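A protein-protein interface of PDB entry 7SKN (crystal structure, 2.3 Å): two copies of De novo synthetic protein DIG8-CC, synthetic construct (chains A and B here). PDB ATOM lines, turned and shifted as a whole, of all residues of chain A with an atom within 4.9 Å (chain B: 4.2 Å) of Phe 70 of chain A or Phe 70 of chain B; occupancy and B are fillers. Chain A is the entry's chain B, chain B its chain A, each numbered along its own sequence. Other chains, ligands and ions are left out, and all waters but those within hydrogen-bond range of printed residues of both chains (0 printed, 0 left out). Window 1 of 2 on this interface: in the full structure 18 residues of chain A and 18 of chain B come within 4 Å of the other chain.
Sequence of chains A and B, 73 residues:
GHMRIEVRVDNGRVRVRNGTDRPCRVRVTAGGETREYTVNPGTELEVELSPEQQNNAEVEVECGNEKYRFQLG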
ATOM      1  N   ILE A   5     -17.943  12.739 -17.446  1.00  0.00           N
ATOM      2  CA  ILE A   5     -17.395  11.575 -18.135  1.00  0.00           C
ATOM      3  C   ILE A   5     -18.516  10.890 -18.903  1.00  0.00           C
ATOM      4  O   ILE A   5     -19.608  10.683 -18.365  1.00  0.00           O
ATOM      5  CB  ILE A   5     -16.730  10.585 -17.157  1.00  0.00           C
ATOM      6  CG1 ILE A   5     -15.544  11.240 -16.451  1.00  0.00           C
ATOM      7  CG2 ILE A   5     -16.270   9.331 -17.886  1.00  0.00           C
ATOM      8  CD1 ILE A   5     -14.827  10.314 -15.505  1.00  0.00           C
ATOM      9  N   VAL A   7     -19.062   7.460 -21.612  1.00  0.00           N
ATOM     10  CA  VAL A   7     -18.492   6.252 -22.200  1.00  0.00           C
ATOM     11  C   VAL A   7     -19.541   5.613 -23.097  1.00  0.00           C
ATOM     12  O   VAL A   7     -20.675   5.380 -22.666  1.00  0.00           O
ATOM     13  CB  VAL A   7     -18.028   5.252 -21.123  1.00  0.00           C
ATOM     14  CG1 VAL A   7     -17.586   3.947 -21.765  1.00  0.00           C
ATOM     15  CG2 VAL A   7     -16.904   5.849 -20.290  1.00  0.00           C
ATOM     16  N   VAL A   9     -20.105   2.356 -25.995  1.00  0.00           N
ATOM     17  CA  VAL A   9     -19.614   1.132 -26.636  1.00  0.00           C
ATOM     18  C   VAL A   9     -20.692   0.674 -27.618  1.00  0.00           C
ATOM     19  O   VAL A   9     -21.623  -0.048 -27.247  1.00  0.00           O
ATOM     20  CB  VAL A   9     -19.285   0.026 -25.628  1.00  0.00           C
ATOM     21  CG1 VAL A   9     -18.617  -1.138 -26.333  1.00  0.00           C
ATOM     22  CG2 VAL A   9     -18.404   0.559 -24.508  1.00  0.00           C
ATOM     23  N   ALA A  57     -16.061  -6.124 -22.260  1.00  0.00           N
ATOM     24  CA  ALA A  57     -15.091  -5.053 -22.103  1.00  0.00           C
ATOM     25  C   ALA A  57     -15.344  -4.265 -20.824  1.00  0.00           C
ATOM     26  O   ALA A  57     -16.478  -4.165 -20.346  1.00  0.00           O
ATOM     27  CB  ALA A  57     -15.125  -4.102 -23.300  1.00  0.00           C
ATOM     28  N   GLU A  58     -14.268  -3.697 -20.285  1.00  0.00           N
ATOM     29  CA  GLU A  58     -14.313  -2.877 -19.084  1.00  0.00           C
ATOM     30  C   GLU A  58     -13.505  -1.612 -19.320  1.00  0.00           C
ATOM     31  O   GLU A  58     -12.364  -1.681 -19.787  1.00  0.00           O
ATOM     32  CB  GLU A  58     -13.769  -3.643 -17.875  1.00  0.00           C
ATOM     33  CG  GLU A  58     -13.516  -2.779 -16.654  1.00  0.00           C
ATOM     34  CD  GLU A  58     -12.892  -3.561 -15.518  1.00  0.00           C
ATOM     35  OE1 GLU A  58     -13.287  -4.729 -15.312  1.00  0.00           O
ATOM     36  OE2 GLU A  58     -11.999  -3.013 -14.839  1.00  0.00           O
ATOM     37  N   VAL A  59     -14.093  -0.463 -18.999  1.00  0.00           N
ATOM     38  CA  VAL A  59     -13.434   0.831 -19.140  1.00  0.00           C
ATOM     39  C   VAL A  59     -13.311   1.447 -17.756  1.00  0.00           C
ATOM     40  O   VAL A  59     -14.321   1.670 -17.078  1.00  0.00           O
ATOM     41  CB  VAL A  59     -14.201   1.765 -20.087  1.00  0.00           C
ATOM     42  CG1 VAL A  59     -13.522   3.124 -20.151  1.00  0.00           C
ATOM     43  CG2 VAL A  59     -14.299   1.147 -21.475  1.00  0.00           C
ATOM     44  N   GLU A  60     -12.081   1.726 -17.341  1.00  0.00           N
ATOM     45  CA  GLU A  60     -11.805   2.376 -16.070  1.00  0.00           C
ATOM     46  C   GLU A  60     -11.210   3.750 -16.336  1.00  0.00           C
ATOM     47  O   GLU A  60     -10.264   3.878 -17.119  1.00  0.00           O
ATOM     48  CB  GLU A  60     -10.853   1.535 -15.216  1.00  0.00           C
ATOM     49  CG  GLU A  60     -10.458   2.184 -13.898  1.00  0.00           C
ATOM     50  CD  GLU A  60      -9.597   1.277 -13.038  1.00  0.00           C
ATOM     51  OE1 GLU A  60      -9.938   0.082 -12.905  1.00  0.00           O
ATOM     52  OE2 GLU A  60      -8.577   1.760 -12.501  1.00  0.00           O
ATOM     53  N   VAL A  61     -11.775   4.770 -15.700  1.00  0.00           N
ATOM     54  CA  VAL A  61     -11.342   6.151 -15.869  1.00  0.00           C
ATOM     55  C   VAL A  61     -10.922   6.688 -14.511  1.00  0.00           C
ATOM     56  O   VAL A  61     -11.661   6.549 -13.529  1.00  0.00           O
ATOM     57  CB  VAL A  61     -12.453   7.024 -16.482  1.00  0.00           C
ATOM     58  CG1 VAL A  61     -11.936   8.430 -16.748  1.00  0.00           C
ATOM     59  CG2 VAL A  61     -12.981   6.392 -17.759  1.00  0.00           C
ATOM     60  N   TYR A  68     -13.896   5.701 -11.631  1.00  0.00           N
ATOM     61  CA  TYR A  68     -15.304   5.412 -11.894  1.00  0.00           C
ATOM     62  C   TYR A  68     -15.542   3.996 -12.404  1.00  0.00           C
ATOM     63  O   TYR A  68     -16.202   3.209 -11.722  1.00  0.00           O
ATOM     64  CB  TYR A  68     -15.836   6.470 -12.870  1.00  0.00           C
ATOM     65  CG  TYR A  68     -15.716   7.863 -12.295  1.00  0.00           C
ATOM     66  CD1 TYR A  68     -16.733   8.393 -11.517  1.00  0.00           C
ATOM     67  CD2 TYR A  68     -14.574   8.630 -12.494  1.00  0.00           C
ATOM     68  CE1 TYR A  68     -16.631   9.651 -10.969  1.00  0.00           C
ATOM     69  CE2 TYR A  68     -14.465   9.898 -11.949  1.00  0.00           C
ATOM     70  CZ  TYR A  68     -15.500  10.399 -11.187  1.00  0.00           C
ATOM     71  OH  TYR A  68     -15.412  11.654 -10.636  1.00  0.00           O
ATOM     72  N   ARG A  69     -14.982   3.630 -13.556  1.00  0.00           N
ATOM     73  CA  ARG A  69     -15.085   2.287 -14.127  1.00  0.00           C
ATOM     74  C   ARG A  69     -16.478   1.974 -14.673  1.00  0.00           C
ATOM     75  O   ARG A  69     -17.484   2.122 -13.973  1.00  0.00           O
ATOM     76  CB  ARG A  69     -14.673   1.213 -13.113  1.00  0.00           C
ATOM     77  CG  ARG A  69     -14.824  -0.205 -13.646  1.00  0.00           C
ATOM     78  CD  ARG A  69     -13.854  -1.170 -12.996  1.00  0.00           C
ATOM     79  NE  ARG A  69     -14.264  -1.516 -11.644  1.00  0.00           N
ATOM     80  CZ  ARG A  69     -13.426  -1.864 -10.678  1.00  0.00           C
ATOM     81  NH1 ARG A  69     -12.117  -1.868 -10.867  1.00  0.00           N
ATOM     82  NH2 ARG A  69     -13.915  -2.212  -9.491  1.00  0.00           N
ATOM     83  N   PHE A  70     -16.540   1.536 -15.929  1.00  0.00           N
ATOM     84  CA  PHE A  70     -17.774   1.099 -16.568  1.00  0.00           C
ATOM     85  C   PHE A  70     -17.501  -0.231 -17.249  1.00  0.00           C
ATOM     86  O   PHE A  70     -16.515  -0.359 -17.980  1.00  0.00           O
ATOM     87  CB  PHE A  70     -18.273   2.125 -17.596  1.00  0.00           C
ATOM     88  CG  PHE A  70     -18.452   3.509 -17.041  1.00  0.00           C
ATOM     89  CD1 PHE A  70     -17.375   4.376 -16.940  1.00  0.00           C
ATOM     90  CD2 PHE A  70     -19.700   3.950 -16.632  1.00  0.00           C
ATOM     91  CE1 PHE A  70     -17.538   5.650 -16.430  1.00  0.00           C
ATOM     92  CE2 PHE A  70     -19.870   5.222 -16.125  1.00  0.00           C
ATOM     93  CZ  PHE A  70     -18.788   6.074 -16.023  1.00  0.00           C
ATOM     94  N   GLN A  71     -18.371  -1.215 -17.025  1.00  0.00           N
ATOM     95  CA  GLN A  71     -18.117  -2.571 -17.490  1.00  0.00           C
ATOM     96  C   GLN A  71     -19.323  -3.142 -18.223  1.00  0.00           C
ATOM     97  O   GLN A  71     -20.463  -3.015 -17.765  1.00  0.00           O
ATOM     98  CB  GLN A  71     -17.745  -3.491 -16.323  1.00  0.00           C
ATOM     99  CG  GLN A  71     -17.267  -4.862 -16.762  1.00  0.00           C
ATOM    100  CD  GLN A  71     -16.636  -5.650 -15.633  1.00  0.00           C
ATOM    101  OE1 GLN A  71     -16.735  -5.275 -14.465  1.00  0.00           O
ATOM    102  NE2 GLN A  71     -15.974  -6.748 -15.980  1.00  0.00           N
ATOM    103  N   LEU A  72     -19.059  -3.781 -19.362  1.00  0.00           N
ATOM    104  CA  LEU A  72     -20.061  -4.512 -20.132  1.00  0.00           C
ATOM    105  C   LEU A  72     -19.637  -5.974 -20.146  1.00  0.00           C
ATOM    106  O   LEU A  72     -18.587  -6.314 -20.699  1.00  0.00           O
ATOM    107  CB  LEU A  72     -20.183  -3.961 -21.553  1.00  0.00           C
ATOM    108  CG  LEU A  72     -21.533  -4.037 -22.276  1.00  0.00           C
ATOM    109  CD1 LEU A  72     -21.368  -3.648 -23.740  1.00  0.00           C
ATOM    110  CD2 LEU A  72     -22.187  -5.407 -22.154  1.00  0.00           C
ATOM    111  N   VAL B   7     -20.635   1.238 -12.786  1.00  0.00           N
ATOM    112  CA  VAL B   7     -21.798   0.788 -13.549  1.00  0.00           C
ATOM    113  C   VAL B   7     -21.430  -0.511 -14.253  1.00  0.00           C
ATOM    114  O   VAL B   7     -20.491  -0.541 -15.057  1.00  0.00           O
ATOM    115  CB  VAL B   7     -22.268   1.842 -14.566  1.00  0.00           C
ATOM    116  CG1 VAL B   7     -23.429   1.298 -15.387  1.00  0.00           C
ATOM    117  CG2 VAL B   7     -22.667   3.129 -13.863  1.00  0.00           C
ATOM    118  N   GLU B  58     -28.961   3.189 -22.107  1.00  0.00           N
ATOM    119  CA  GLU B  58     -28.185   4.306 -21.588  1.00  0.00           C
ATOM    120  C   GLU B  58     -28.418   4.413 -20.090  1.00  0.00           C
ATOM    121  O   GLU B  58     -29.553   4.276 -19.623  1.00  0.00           O
ATOM    122  CB  GLU B  58     -28.571   5.609 -22.294  1.00  0.00           C
ATOM    123  CG  GLU B  58     -28.174   6.877 -21.567  1.00  0.00           C
ATOM    124  CD  GLU B  58     -28.647   8.115 -22.298  1.00  0.00           C
ATOM    125  OE1 GLU B  58     -28.586   8.122 -23.546  1.00  0.00           O
ATOM    126  OE2 GLU B  58     -29.093   9.073 -21.632  1.00  0.00           O
ATOM    127  N   VAL B  59     -27.339   4.635 -19.345  1.00  0.00           N
ATOM    128  CA  VAL B  59     -27.392   4.825 -17.901  1.00  0.00           C
ATOM    129  C   VAL B  59     -26.745   6.167 -17.593  1.00  0.00           C
ATOM    130  O   VAL B  59     -25.587   6.403 -17.960  1.00  0.00           O
ATOM    131  CB  VAL B  59     -26.686   3.686 -17.147  1.00  0.00           C
ATOM    132  CG1 VAL B  59     -26.792   3.889 -15.644  1.00  0.00           C
ATOM    133  CG2 VAL B  59     -27.274   2.339 -17.548  1.00  0.00           C
ATOM    134  N   ARG B  69     -22.494   9.433 -17.930  1.00  0.00           N
ATOM    135  CA  ARG B  69     -23.361   8.684 -18.828  1.00  0.00           C
ATOM    136  C   ARG B  69     -22.615   7.490 -19.403  1.00  0.00           C
ATOM    137  O   ARG B  69     -21.443   7.595 -19.776  1.00  0.00           O
ATOM    138  CB  ARG B  69     -23.891   9.574 -19.959  1.00  0.00           C
ATOM    139  CG  ARG B  69     -25.047   8.970 -20.735  1.00  0.00           C
ATOM    140  CD  ARG B  69     -25.887  10.058 -21.390  1.00  0.00           C
ATOM    141  NE  ARG B  69     -25.119  10.839 -22.351  1.00  0.00           N
ATOM    142  CZ  ARG B  69     -25.517  11.995 -22.867  1.00  0.00           C
ATOM    143  NH1 ARG B  69     -26.666  12.548 -22.516  1.00  0.00           N
ATOM    144  NH2 ARG B  69     -24.741  12.611 -23.754  1.00  0.00           N
ATOM    145  N   PHE B  70     -23.307   6.354 -19.467  1.00  0.00           N
ATOM    146  CA  PHE B  70     -22.776   5.117 -20.026  1.00  0.00           C
ATOM    147  C   PHE B  70     -23.757   4.626 -21.078  1.00  0.00           C
ATOM    148  O   PHE B  70     -24.931   4.398 -20.771  1.00  0.00           O
ATOM    149  CB  PHE B  70     -22.578   4.063 -18.930  1.00  0.00           C
ATOM    150  CG  PHE B  70     -21.883   2.813 -19.395  1.00  0.00           C
ATOM    151  CD1 PHE B  70     -21.103   2.815 -20.537  1.00  0.00           C
ATOM    152  CD2 PHE B  70     -22.014   1.631 -18.685  1.00  0.00           C
ATOM    153  CE1 PHE B  70     -20.466   1.662 -20.961  1.00  0.00           C
ATOM    154  CE2 PHE B  70     -21.381   0.478 -19.106  1.00  0.00           C
ATOM    155  CZ  PHE B  70     -20.607   0.495 -20.245  1.00  0.00           C
ATOM    156  N   GLN B  71     -23.285   4.459 -22.311  1.00  0.00           N
ATOM    157  CA  GLN B  71     -24.142   4.062 -23.417  1.00  0.00           C
ATOM    158  C   GLN B  71     -23.741   2.692 -23.942  1.00  0.00           C
ATOM    159  O   GLN B  71     -22.552   2.376 -24.047  1.00  0.00           O
ATOM    160  CB  GLN B  71     -24.096   5.076 -24.560  1.00  0.00           C
ATOM    161  CG  GLN B  71     -24.704   6.422 -24.223  1.00  0.00           C
ATOM    162  CD  GLN B  71     -24.870   7.301 -25.444  1.00  0.00           C
ATOM    163  OE1 GLN B  71     -24.875   6.818 -26.577  1.00  0.00           O
ATOM    164  NE2 GLN B  71     -25.004   8.602 -25.220  1.00  0.00           N
ATOM    165  N   LEU B  72     -24.747   1.890 -24.275  1.00  0.00           N
ATOM    166  CA  LEU B  72     -24.571   0.573 -24.879  1.00  0.00           C
ATOM    167  C   LEU B  72     -25.281   0.600 -26.229  1.00  0.00           C
ATOM    168  O   LEU B  72     -26.508   0.480 -26.292  1.00  0.00           O
ATOM    169  CB  LEU B  72     -25.127  -0.519 -23.976  1.00  0.00           C
ATOM    170  CG  LEU B  72     -24.760  -0.401 -22.499  1.00  0.00           C
ATOM    171  CD1 LEU B  72     -25.675  -1.274 -21.656  1.00  0.00           C
ATOM    172  CD2 LEU B  72     -23.306  -0.778 -22.286  1.00  0.00           C
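Val 7 of chain A touches Arg 69 of chain B, and with the chains exchanged Arg 69 of chain A touches Val 7 of chain B. Val 7 of chain A touches Phe 70 of chain B, and with the chains exchanged Phe 70 of chain A touches Val 7 of chain B. Gln 71 of chain A touches Phe 70 of chain B, but with the chains exchanged Phe 70 of chain A does not touch Gln 71 of chain B (6.7 Å). Leu 72 of chain B touches its own counterpart, Leu 72 of chain A.
Of the 7 printed residues of chain B, 5 touch a printed residue of chain A. Printed residues of chain A that touch a printed residue of chain B: Ile 5, Val 7, Val 9, Arg 69, Phe 70, Gln 71 and Leu 72. Hydrophobic or aromatic side chains of chain A that line the printed part of chain B: Val 7, Phe 70 and Leu 72. Among the printed residues, 12 pairs touch across the chains.
The backbone NH (N) of Val 7 of chain B lies within hydrogen-bond range of the backbone carbonyl oxygen (O) of Arg 69 of chain A (3.5 Å). O of Val 7 of chain B lies within hydrogen-bond range of N of Gln 71 of chain A, 3.0 Å away. The backbone carbonyl oxygen (O) of Ile 5 of chain A lies within hydrogen-bond range of the backbone NH (N) of Arg 69 of chain B (3.2 Å). The backbone carbonyl oxygen of Arg 69 of chain B lies within hydrogen-bond range of the backbone NH of Val 7 of chain A (3.0 Å). The backbone NH (N) of Gln 71 of chain B is in hydrogen-bond range of the backbone carbonyl oxygen (O) of Val 7 of chain A, at 2.8 Å. The backbone carbonyl oxygen (O) of Gln 71 of chain B lies within hydrogen-bond range of the backbone NH (N) of Val 9 of chain A (3.1 Å).
Of the printed residues of chain B, Val 9 of chain A touches Gln 71 and Leu 72. Tyr 68 of chain A touches none of the printed residues of chain B. Of the printed residues of chain B, Arg 69 of chain A touches Val 7. Phe 70 of chain A touches just these residues of chain B: Val 7 (3.5 Å) and Phe 70 (3.7 Å). Printed residues of chain B within 4 Å of Leu 72 of chain A: Leu 72 (3.7 Å). Of the printed residues of chain A, Val 7 of chain B touches Arg 69 (3.5 Å), Phe 70 (3.5 Å) and Gln 71 (3.0 Å). Val 59 of chain B touches none of the printed residues of chain A. Of the printed residues of chain A, Arg 69 of chain B touches Ile 5 (3.2 Å) and Val 7 (3.0 Å). The nearest printed residue of chain B that does not touch Phe 70 of chain A is Arg 69 of chain B (4.6 Å). The nearest residue of chain A that does not touch Phe 70 of chain B is Val 9 of chain A (4.2 Å).
The backbone carbonyl oxygen of Val 59 of chain B sits at hydrogen-bond distance from the backbone NH of Phe 70 of chain B. O of Ala 57 of chain A is in hydrogen-bond range of N of Leu 72 of chain A (2.8 Å). The side-chain carboxylate (OE1) of Glu 58 of chain A is in hydrogen-bond range of the side-chain amide nitrogen (NE2) of Gln 71 of chain A. The backbone carbonyl oxygen (O) of Val 59 of chain A sits at hydrogen-bond distance from the backbone NH (N) of Phe 70 of chain A (2.5 Å). NH1 of Arg 69 of chain A lies within salt-bridge range of OE1 of Glu 60 of chain A (3.6 Å).
Among the printed residues, merely in contact across the chains: Val 7 of chain A with Phe 70 of chain B (3.4 Å), Val 9 of chain A with Leu 72 of chain B (3.8 Å), Phe 70 of chain A with Val 7 of chain B (3.5 Å), Phe 70 of chain A with Phe 70 of chain B (3.7 Å), Gln 71 of chain A with Phe 70 of chain B (3.9 Å) and Leu 72 of chain A with Leu 72 of chain B (3.7 Å).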
